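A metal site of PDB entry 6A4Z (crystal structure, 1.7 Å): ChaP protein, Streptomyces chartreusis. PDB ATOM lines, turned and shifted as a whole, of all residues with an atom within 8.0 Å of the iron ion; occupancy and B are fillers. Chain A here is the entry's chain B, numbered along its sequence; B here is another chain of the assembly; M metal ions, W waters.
The backbone carbonyl oxygen (O) of His 10 of chain B sits at hydrogen-bond distance from the backbone NH (N) of Ala 68 (3.0 Å).
A ring nitrogen (ND1) of His 10 of chain B sits at hydrogen-bond distance from the side-chain amide oxygen (OD1) of Asn 9 of chain B (2.8 Å).
The side-chain hydroxyl (OH) of Tyr 112 lies within hydrogen-bond range of the side-chain carboxylate (OE2) of Glu 122, at 3.4 Å.
The backbone NH of Glu 122 is in hydrogen-bond range of the backbone carbonyl oxygen of Cys 67.
O of Glu 122 sits at hydrogen-bond distance from N of Phe 69.
N of Ile 12 of chain B sits at hydrogen-bond distance from O of His 66 (3.0 Å).
The backbone carbonyl oxygen (O) of Asn 120 lies within hydrogen-bond range of a ring nitrogen (ND1) of His 66, at 2.7 Å.
O of His 66 lies within hydrogen-bond range of OG1 of Thr 11 of chain B (2.9 Å).
Four residues have an atom within 4 Å of the iron ion: His 66, Glu 122, Tyr 128 and His 10 of chain B.
Along chain A the residues within 4 Å of the iron ion span positions 66 to 128.
The nearest printed residue that does not touch the iron ion is Tyr 112 (4.2 Å).
Water W1 binds the iron ion (2.2 Å).
A ring nitrogen (NE2) of His 10 of chain B binds the iron ion, at 2.2 Å.
The iron ion is bound by OE1 of Glu 122, at 2.2 Å.
Water W2 is bound to the iron ion.
The iron ion is bound by the side-chain hydroxyl (OH) of Tyr 128 (2.3 Å).
The iron ion is bound by NE2 of His 66, 2.3 Å away.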
ATOM      1  N   HIS A  66      -9.428 -12.478  19.590  1.00  0.00           N
ATOM      2  CA  HIS A  66      -9.108 -13.518  18.619  1.00  0.00           C
ATOM      3  C   HIS A  66     -10.333 -14.389  18.402  1.00  0.00           C
ATOM      4  O   HIS A  66     -10.859 -14.954  19.364  1.00  0.00           O
ATOM      5  CB  HIS A  66      -7.938 -14.363  19.109  1.00  0.00           C
ATOM      6  CG  HIS A  66      -7.600 -15.501  18.192  1.00  0.00           C
ATOM      7  ND1 HIS A  66      -7.403 -15.329  16.841  1.00  0.00           N
ATOM      8  CD2 HIS A  66      -7.389 -16.819  18.441  1.00  0.00           C
ATOM      9  CE1 HIS A  66      -7.091 -16.491  16.286  1.00  0.00           C
ATOM     10  NE2 HIS A  66      -7.070 -17.409  17.239  1.00  0.00           N
ATOM     11  N   CYS A  67     -10.766 -14.487  17.155  1.00  0.00           N
ATOM     12  CA  CYS A  67     -11.796 -15.429  16.729  1.00  0.00           C
ATOM     13  C   CYS A  67     -11.253 -16.198  15.544  1.00  0.00           C
ATOM     14  O   CYS A  67     -10.602 -15.631  14.669  1.00  0.00           O
ATOM     15  CB  CYS A  67     -13.096 -14.728  16.327  1.00  0.00           C
ATOM     16  SG  CYS A  67     -13.822 -13.781  17.660  1.00  0.00           S
ATOM     17  N   ALA A  68     -11.497 -17.505  15.528  1.00  0.00           N
ATOM     18  CA  ALA A  68     -11.002 -18.354  14.453  1.00  0.00           C
ATOM     19  C   ALA A  68     -12.170 -19.138  13.877  1.00  0.00           C
ATOM     20  O   ALA A  68     -13.035 -19.603  14.623  1.00  0.00           O
ATOM     21  CB  ALA A  68      -9.949 -19.305  14.963  1.00  0.00           C
ATOM     22  N   PHE A  69     -12.174 -19.297  12.555  1.00  0.00           N
ATOM     23  CA  PHE A  69     -13.279 -19.903  11.840  1.00  0.00           C
ATOM     24  C   PHE A  69     -12.801 -21.121  11.062  1.00  0.00           C
ATOM     25  O   PHE A  69     -11.815 -21.059  10.327  1.00  0.00           O
ATOM     26  CB  PHE A  69     -13.922 -18.878  10.900  1.00  0.00           C
ATOM     27  CG  PHE A  69     -14.340 -17.624  11.596  1.00  0.00           C
ATOM     28  CD1 PHE A  69     -15.611 -17.526  12.172  1.00  0.00           C
ATOM     29  CD2 PHE A  69     -13.445 -16.562  11.776  1.00  0.00           C
ATOM     30  CE1 PHE A  69     -16.000 -16.373  12.848  1.00  0.00           C
ATOM     31  CE2 PHE A  69     -13.839 -15.416  12.464  1.00  0.00           C
ATOM     32  CZ  PHE A  69     -15.123 -15.331  13.009  1.00  0.00           C
ATOM     33  N   GLN A  94       0.021 -16.052  14.008  1.00  0.00           N
ATOM     34  CA  GLN A  94      -0.770 -15.220  14.907  1.00  0.00           C
ATOM     35  C   GLN A  94      -0.068 -13.917  15.270  1.00  0.00           C
ATOM     36  O   GLN A  94      -0.749 -12.954  15.659  1.00  0.00           O
ATOM     37  CB  GLN A  94      -1.091 -15.991  16.191  1.00  0.00           C
ATOM     38  CG  GLN A  94       0.155 -16.312  17.007  1.00  0.00           C
ATOM     39  CD  GLN A  94      -0.137 -17.198  18.196  1.00  0.00           C
ATOM     40  OE1 GLN A  94      -0.944 -16.852  19.058  1.00  0.00           O
ATOM     41  NE2 GLN A  94       0.531 -18.349  18.257  1.00  0.00           N
ATOM     42  N   ARG A 105      -0.370 -25.513   9.137  1.00  0.00           N
ATOM     43  CA  ARG A 105      -0.582 -26.159  10.432  1.00  0.00           C
ATOM     44  C   ARG A 105      -1.532 -27.338  10.288  1.00  0.00           C
ATOM     45  O   ARG A 105      -2.562 -27.238   9.619  1.00  0.00           O
ATOM     46  CB  ARG A 105      -1.139 -25.143  11.433  1.00  0.00           C
ATOM     47  CG  ARG A 105      -1.223 -25.648  12.861  1.00  0.00           C
ATOM     48  CD  ARG A 105      -1.493 -24.497  13.809  1.00  0.00           C
ATOM     49  NE  ARG A 105      -1.759 -24.949  15.176  1.00  0.00           N
ATOM     50  CZ  ARG A 105      -1.898 -24.121  16.215  1.00  0.00           C
ATOM     51  NH1 ARG A 105      -1.794 -22.808  16.037  1.00  0.00           N
ATOM     52  NH2 ARG A 105      -2.133 -24.604  17.426  1.00  0.00           N
ATOM     53  N   TYR A 112      -4.246 -15.452   8.944  1.00  0.00           N
ATOM     54  CA  TYR A 112      -4.738 -14.466   9.891  1.00  0.00           C
ATOM     55  C   TYR A 112      -4.947 -13.137   9.175  1.00  0.00           C
ATOM     56  O   TYR A 112      -4.259 -12.821   8.210  1.00  0.00           O
ATOM     57  CB  TYR A 112      -3.767 -14.259  11.056  1.00  0.00           C
ATOM     58  CG  TYR A 112      -3.552 -15.468  11.947  1.00  0.00           C
ATOM     59  CD1 TYR A 112      -2.671 -16.481  11.586  1.00  0.00           C
ATOM     60  CD2 TYR A 112      -4.195 -15.570  13.189  1.00  0.00           C
ATOM     61  CE1 TYR A 112      -2.455 -17.569  12.392  1.00  0.00           C
ATOM     62  CE2 TYR A 112      -3.983 -16.654  14.012  1.00  0.00           C
ATOM     63  CZ  TYR A 112      -3.123 -17.657  13.603  1.00  0.00           C
ATOM     64  OH  TYR A 112      -2.898 -18.744  14.405  1.00  0.00           O
ATOM     65  N   ASN A 120      -7.734 -10.057  15.997  1.00  0.00           N
ATOM     66  CA  ASN A 120      -6.903 -11.019  15.276  1.00  0.00           C
ATOM     67  C   ASN A 120      -7.810 -12.152  14.787  1.00  0.00           C
ATOM     68  O   ASN A 120      -8.180 -13.046  15.547  1.00  0.00           O
ATOM     69  CB  ASN A 120      -5.771 -11.537  16.163  1.00  0.00           C
ATOM     70  CG  ASN A 120      -4.653 -12.210  15.354  1.00  0.00           C
ATOM     71  OD1 ASN A 120      -4.628 -12.155  14.119  1.00  0.00           O
ATOM     72  ND2 ASN A 120      -3.706 -12.813  16.057  1.00  0.00           N
ATOM     73  N   MET A 121      -8.181 -12.086  13.523  1.00  0.00           N
ATOM     74  CA  MET A 121      -9.095 -13.076  12.957  1.00  0.00           C
ATOM     75  C   MET A 121      -8.293 -14.174  12.256  1.00  0.00           C
ATOM     76  O   MET A 121      -7.190 -13.950  11.780  1.00  0.00           O
ATOM     77  CB  MET A 121     -10.078 -12.404  11.978  1.00  0.00           C
ATOM     78  CG  MET A 121     -10.889 -11.272  12.587  1.00  0.00           C
ATOM     79  SD  MET A 121     -11.834 -11.807  14.241  1.00  0.00           S
ATOM     80  CE  MET A 121     -13.045 -10.283  14.451  1.00  0.00           C
ATOM     81  N   GLU A 122      -8.859 -15.381  12.214  1.00  0.00           N
ATOM     82  CA  GLU A 122      -8.153 -16.537  11.662  1.00  0.00           C
ATOM     83  C   GLU A 122      -9.142 -17.435  10.934  1.00  0.00           C
ATOM     84  O   GLU A 122     -10.262 -17.648  11.400  1.00  0.00           O
ATOM     85  CB  GLU A 122      -7.441 -17.296  12.785  1.00  0.00           C
ATOM     86  CG  GLU A 122      -6.810 -18.603  12.372  1.00  0.00           C
ATOM     87  CD  GLU A 122      -6.313 -19.407  13.550  1.00  0.00           C
ATOM     88  OE1 GLU A 122      -6.604 -19.027  14.695  1.00  0.00           O
ATOM     89  OE2 GLU A 122      -5.611 -20.417  13.328  1.00  0.00           O
ATOM     90  N   ILE A 123      -8.726 -17.935   9.763  1.00  0.00           N
ATOM     91  CA  ILE A 123      -9.499 -18.962   9.091  1.00  0.00           C
ATOM     92  C   ILE A 123      -8.602 -20.178   8.920  1.00  0.00           C
ATOM     93  O   ILE A 123      -7.390 -20.072   8.755  1.00  0.00           O
ATOM     94  CB  ILE A 123     -10.081 -18.519   7.734  1.00  0.00           C
ATOM     95  CG1 ILE A 123      -8.977 -17.991   6.816  1.00  0.00           C
ATOM     96  CG2 ILE A 123     -11.149 -17.447   7.949  1.00  0.00           C
ATOM     97  CD1 ILE A 123      -9.439 -17.756   5.386  1.00  0.00           C
ATOM     98  N   MET A 124      -9.238 -21.355   8.971  1.00  0.00           N
ATOM     99  CA  MET A 124      -8.508 -22.617   8.937  1.00  0.00           C
ATOM    100  C   MET A 124      -9.375 -23.679   8.297  1.00  0.00           C
ATOM    101  O   MET A 124     -10.605 -23.602   8.365  1.00  0.00           O
ATOM    102  CB  MET A 124      -8.145 -23.042  10.345  1.00  0.00           C
ATOM    103  CG  MET A 124      -9.393 -23.287  11.163  1.00  0.00           C
ATOM    104  SD  MET A 124      -9.060 -22.913  13.010  1.00  0.00           S
ATOM    105  CE  MET A 124      -7.441 -23.965  13.130  1.00  0.00           C
ATOM    106  N   TYR A 128      -7.093 -27.708  15.215  1.00  0.00           N
ATOM    107  CA  TYR A 128      -5.759 -27.872  15.799  1.00  0.00           C
ATOM    108  C   TYR A 128      -5.541 -29.321  16.201  1.00  0.00           C
ATOM    109  O   TYR A 128      -6.423 -29.980  16.763  1.00  0.00           O
ATOM    110  CB  TYR A 128      -5.607 -26.979  17.036  1.00  0.00           C
ATOM    111  CG  TYR A 128      -5.530 -25.503  16.737  1.00  0.00           C
ATOM    112  CD1 TYR A 128      -5.110 -25.045  15.499  1.00  0.00           C
ATOM    113  CD2 TYR A 128      -5.906 -24.573  17.696  1.00  0.00           C
ATOM    114  CE1 TYR A 128      -5.034 -23.686  15.236  1.00  0.00           C
ATOM    115  CE2 TYR A 128      -5.850 -23.223  17.436  1.00  0.00           C
ATOM    116  CZ  TYR A 128      -5.428 -22.779  16.200  1.00  0.00           C
ATOM    117  OH  TYR A 128      -5.367 -21.423  15.928  1.00  0.00           O
ATOM    118  N   ASN B   9     -14.602 -21.678  15.549  1.00  0.00           N
ATOM    119  CA  ASN B   9     -13.876 -22.795  16.120  1.00  0.00           C
ATOM    120  C   ASN B   9     -13.296 -22.489  17.500  1.00  0.00           C
ATOM    121  O   ASN B   9     -13.289 -23.358  18.375  1.00  0.00           O
ATOM    122  CB  ASN B   9     -12.754 -23.240  15.170  1.00  0.00           C
ATOM    123  CG  ASN B   9     -11.984 -24.428  15.684  1.00  0.00           C
ATOM    124  OD1 ASN B   9     -10.934 -24.274  16.300  1.00  0.00           O
ATOM    125  ND2 ASN B   9     -12.518 -25.619  15.466  1.00  0.00           N
ATOM    126  N   HIS B  10     -12.775 -21.290  17.689  1.00  0.00           N
ATOM    127  CA  HIS B  10     -12.320 -20.901  19.016  1.00  0.00           C
ATOM    128  C   HIS B  10     -12.320 -19.391  19.120  1.00  0.00           C
ATOM    129  O   HIS B  10     -12.351 -18.670  18.124  1.00  0.00           O
ATOM    130  CB  HIS B  10     -10.948 -21.492  19.370  1.00  0.00           C
ATOM    131  CG  HIS B  10      -9.847 -21.214  18.393  1.00  0.00           C
ATOM    132  ND1 HIS B  10      -9.564 -22.050  17.335  1.00  0.00           N
ATOM    133  CD2 HIS B  10      -8.930 -20.219  18.343  1.00  0.00           C
ATOM    134  CE1 HIS B  10      -8.525 -21.573  16.661  1.00  0.00           C
ATOM    135  NE2 HIS B  10      -8.116 -20.466  17.258  1.00  0.00           N
ATOM    136  N   THR B  11     -12.363 -18.925  20.367  1.00  0.00           N
ATOM    137  CA  THR B  11     -12.236 -17.505  20.650  1.00  0.00           C
ATOM    138  C   THR B  11     -11.502 -17.372  21.965  1.00  0.00           C
ATOM    139  O   THR B  11     -11.603 -18.232  22.846  1.00  0.00           O
ATOM    140  CB  THR B  11     -13.586 -16.797  20.685  1.00  0.00           C
ATOM    141  OG1 THR B  11     -13.373 -15.383  20.791  1.00  0.00           O
ATOM    142  CG2 THR B  11     -14.424 -17.281  21.864  1.00  0.00           C
ATOM    143  N   ILE B  12     -10.701 -16.311  22.082  1.00  0.00           N
ATOM    144  CA  ILE B  12      -9.914 -16.070  23.279  1.00  0.00           C
ATOM    145  C   ILE B  12     -10.714 -15.226  24.258  1.00  0.00           C
ATOM    146  O   ILE B  12     -11.376 -14.256  23.866  1.00  0.00           O
ATOM    147  CB  ILE B  12      -8.589 -15.368  22.934  1.00  0.00           C
ATOM    148  CG1 ILE B  12      -7.609 -16.345  22.302  1.00  0.00           C
ATOM    149  CG2 ILE B  12      -7.967 -14.721  24.169  1.00  0.00           C
ATOM    150  CD1 ILE B  12      -6.334 -15.675  21.813  1.00  0.00           C
ATOM    151  N   MET B  37      -2.945 -25.542  26.228  1.00  0.00           N
ATOM    152  CA  MET B  37      -2.398 -25.411  24.894  1.00  0.00           C
ATOM    153  C   MET B  37      -1.668 -24.083  24.775  1.00  0.00           C
ATOM    154  O   MET B  37      -2.295 -23.032  24.649  1.00  0.00           O
ATOM    155  CB  MET B  37      -3.493 -25.499  23.833  1.00  0.00           C
ATOM    156  CG  MET B  37      -2.975 -25.344  22.411  1.00  0.00           C
ATOM    157  SD  MET B  37      -4.359 -24.979  21.085  1.00  0.00           S
ATOM    158  CE  MET B  37      -5.044 -23.304  21.813  1.00  0.00           C
ATOM    159  N   PHE B  40      -2.821 -21.036  26.768  1.00  0.00           N
ATOM    160  CA  PHE B  40      -4.269 -21.107  26.923  1.00  0.00           C
ATOM    161  C   PHE B  40      -4.698 -22.231  27.849  1.00  0.00           C
ATOM    162  O   PHE B  40      -4.064 -23.286  27.942  1.00  0.00           O
ATOM    163  CB  PHE B  40      -4.948 -21.300  25.552  1.00  0.00           C
ATOM    164  CG  PHE B  40      -4.612 -20.222  24.559  1.00  0.00           C
ATOM    165  CD1 PHE B  40      -5.136 -18.949  24.715  1.00  0.00           C
ATOM    166  CD2 PHE B  40      -3.741 -20.464  23.504  1.00  0.00           C
ATOM    167  CE1 PHE B  40      -4.843 -17.953  23.814  1.00  0.00           C
ATOM    168  CE2 PHE B  40      -3.419 -19.459  22.597  1.00  0.00           C
ATOM    169  CZ  PHE B  40      -3.963 -18.195  22.755  1.00  0.00           C
ATOM    170  N   ASP B  52     -10.818 -20.168  24.739  1.00  0.00           N
ATOM    171  CA  ASP B  52      -9.406 -20.327  25.053  1.00  0.00           C
ATOM    172  C   ASP B  52      -9.041 -19.227  26.048  1.00  0.00           C
ATOM    173  O   ASP B  52      -8.826 -18.084  25.658  1.00  0.00           O
ATOM    174  CB  ASP B  52      -8.567 -20.264  23.783  1.00  0.00           C
ATOM    175  CG  ASP B  52      -8.986 -21.317  22.768  1.00  0.00           C
ATOM    176  OD1 ASP B  52      -9.865 -22.156  23.096  1.00  0.00           O
ATOM    177  OD2 ASP B  52      -8.467 -21.291  21.636  1.00  0.00           O
HETATM  178 FE    FE M   1      -6.206 -19.494  16.805  1.00  0.00          FE
HETATM  179  O   HOH W   1      -5.435 -19.790  18.809  1.00  0.00           O
HETATM  180  O   HOH W   2      -4.097 -18.818  16.823  1.00  0.00           O
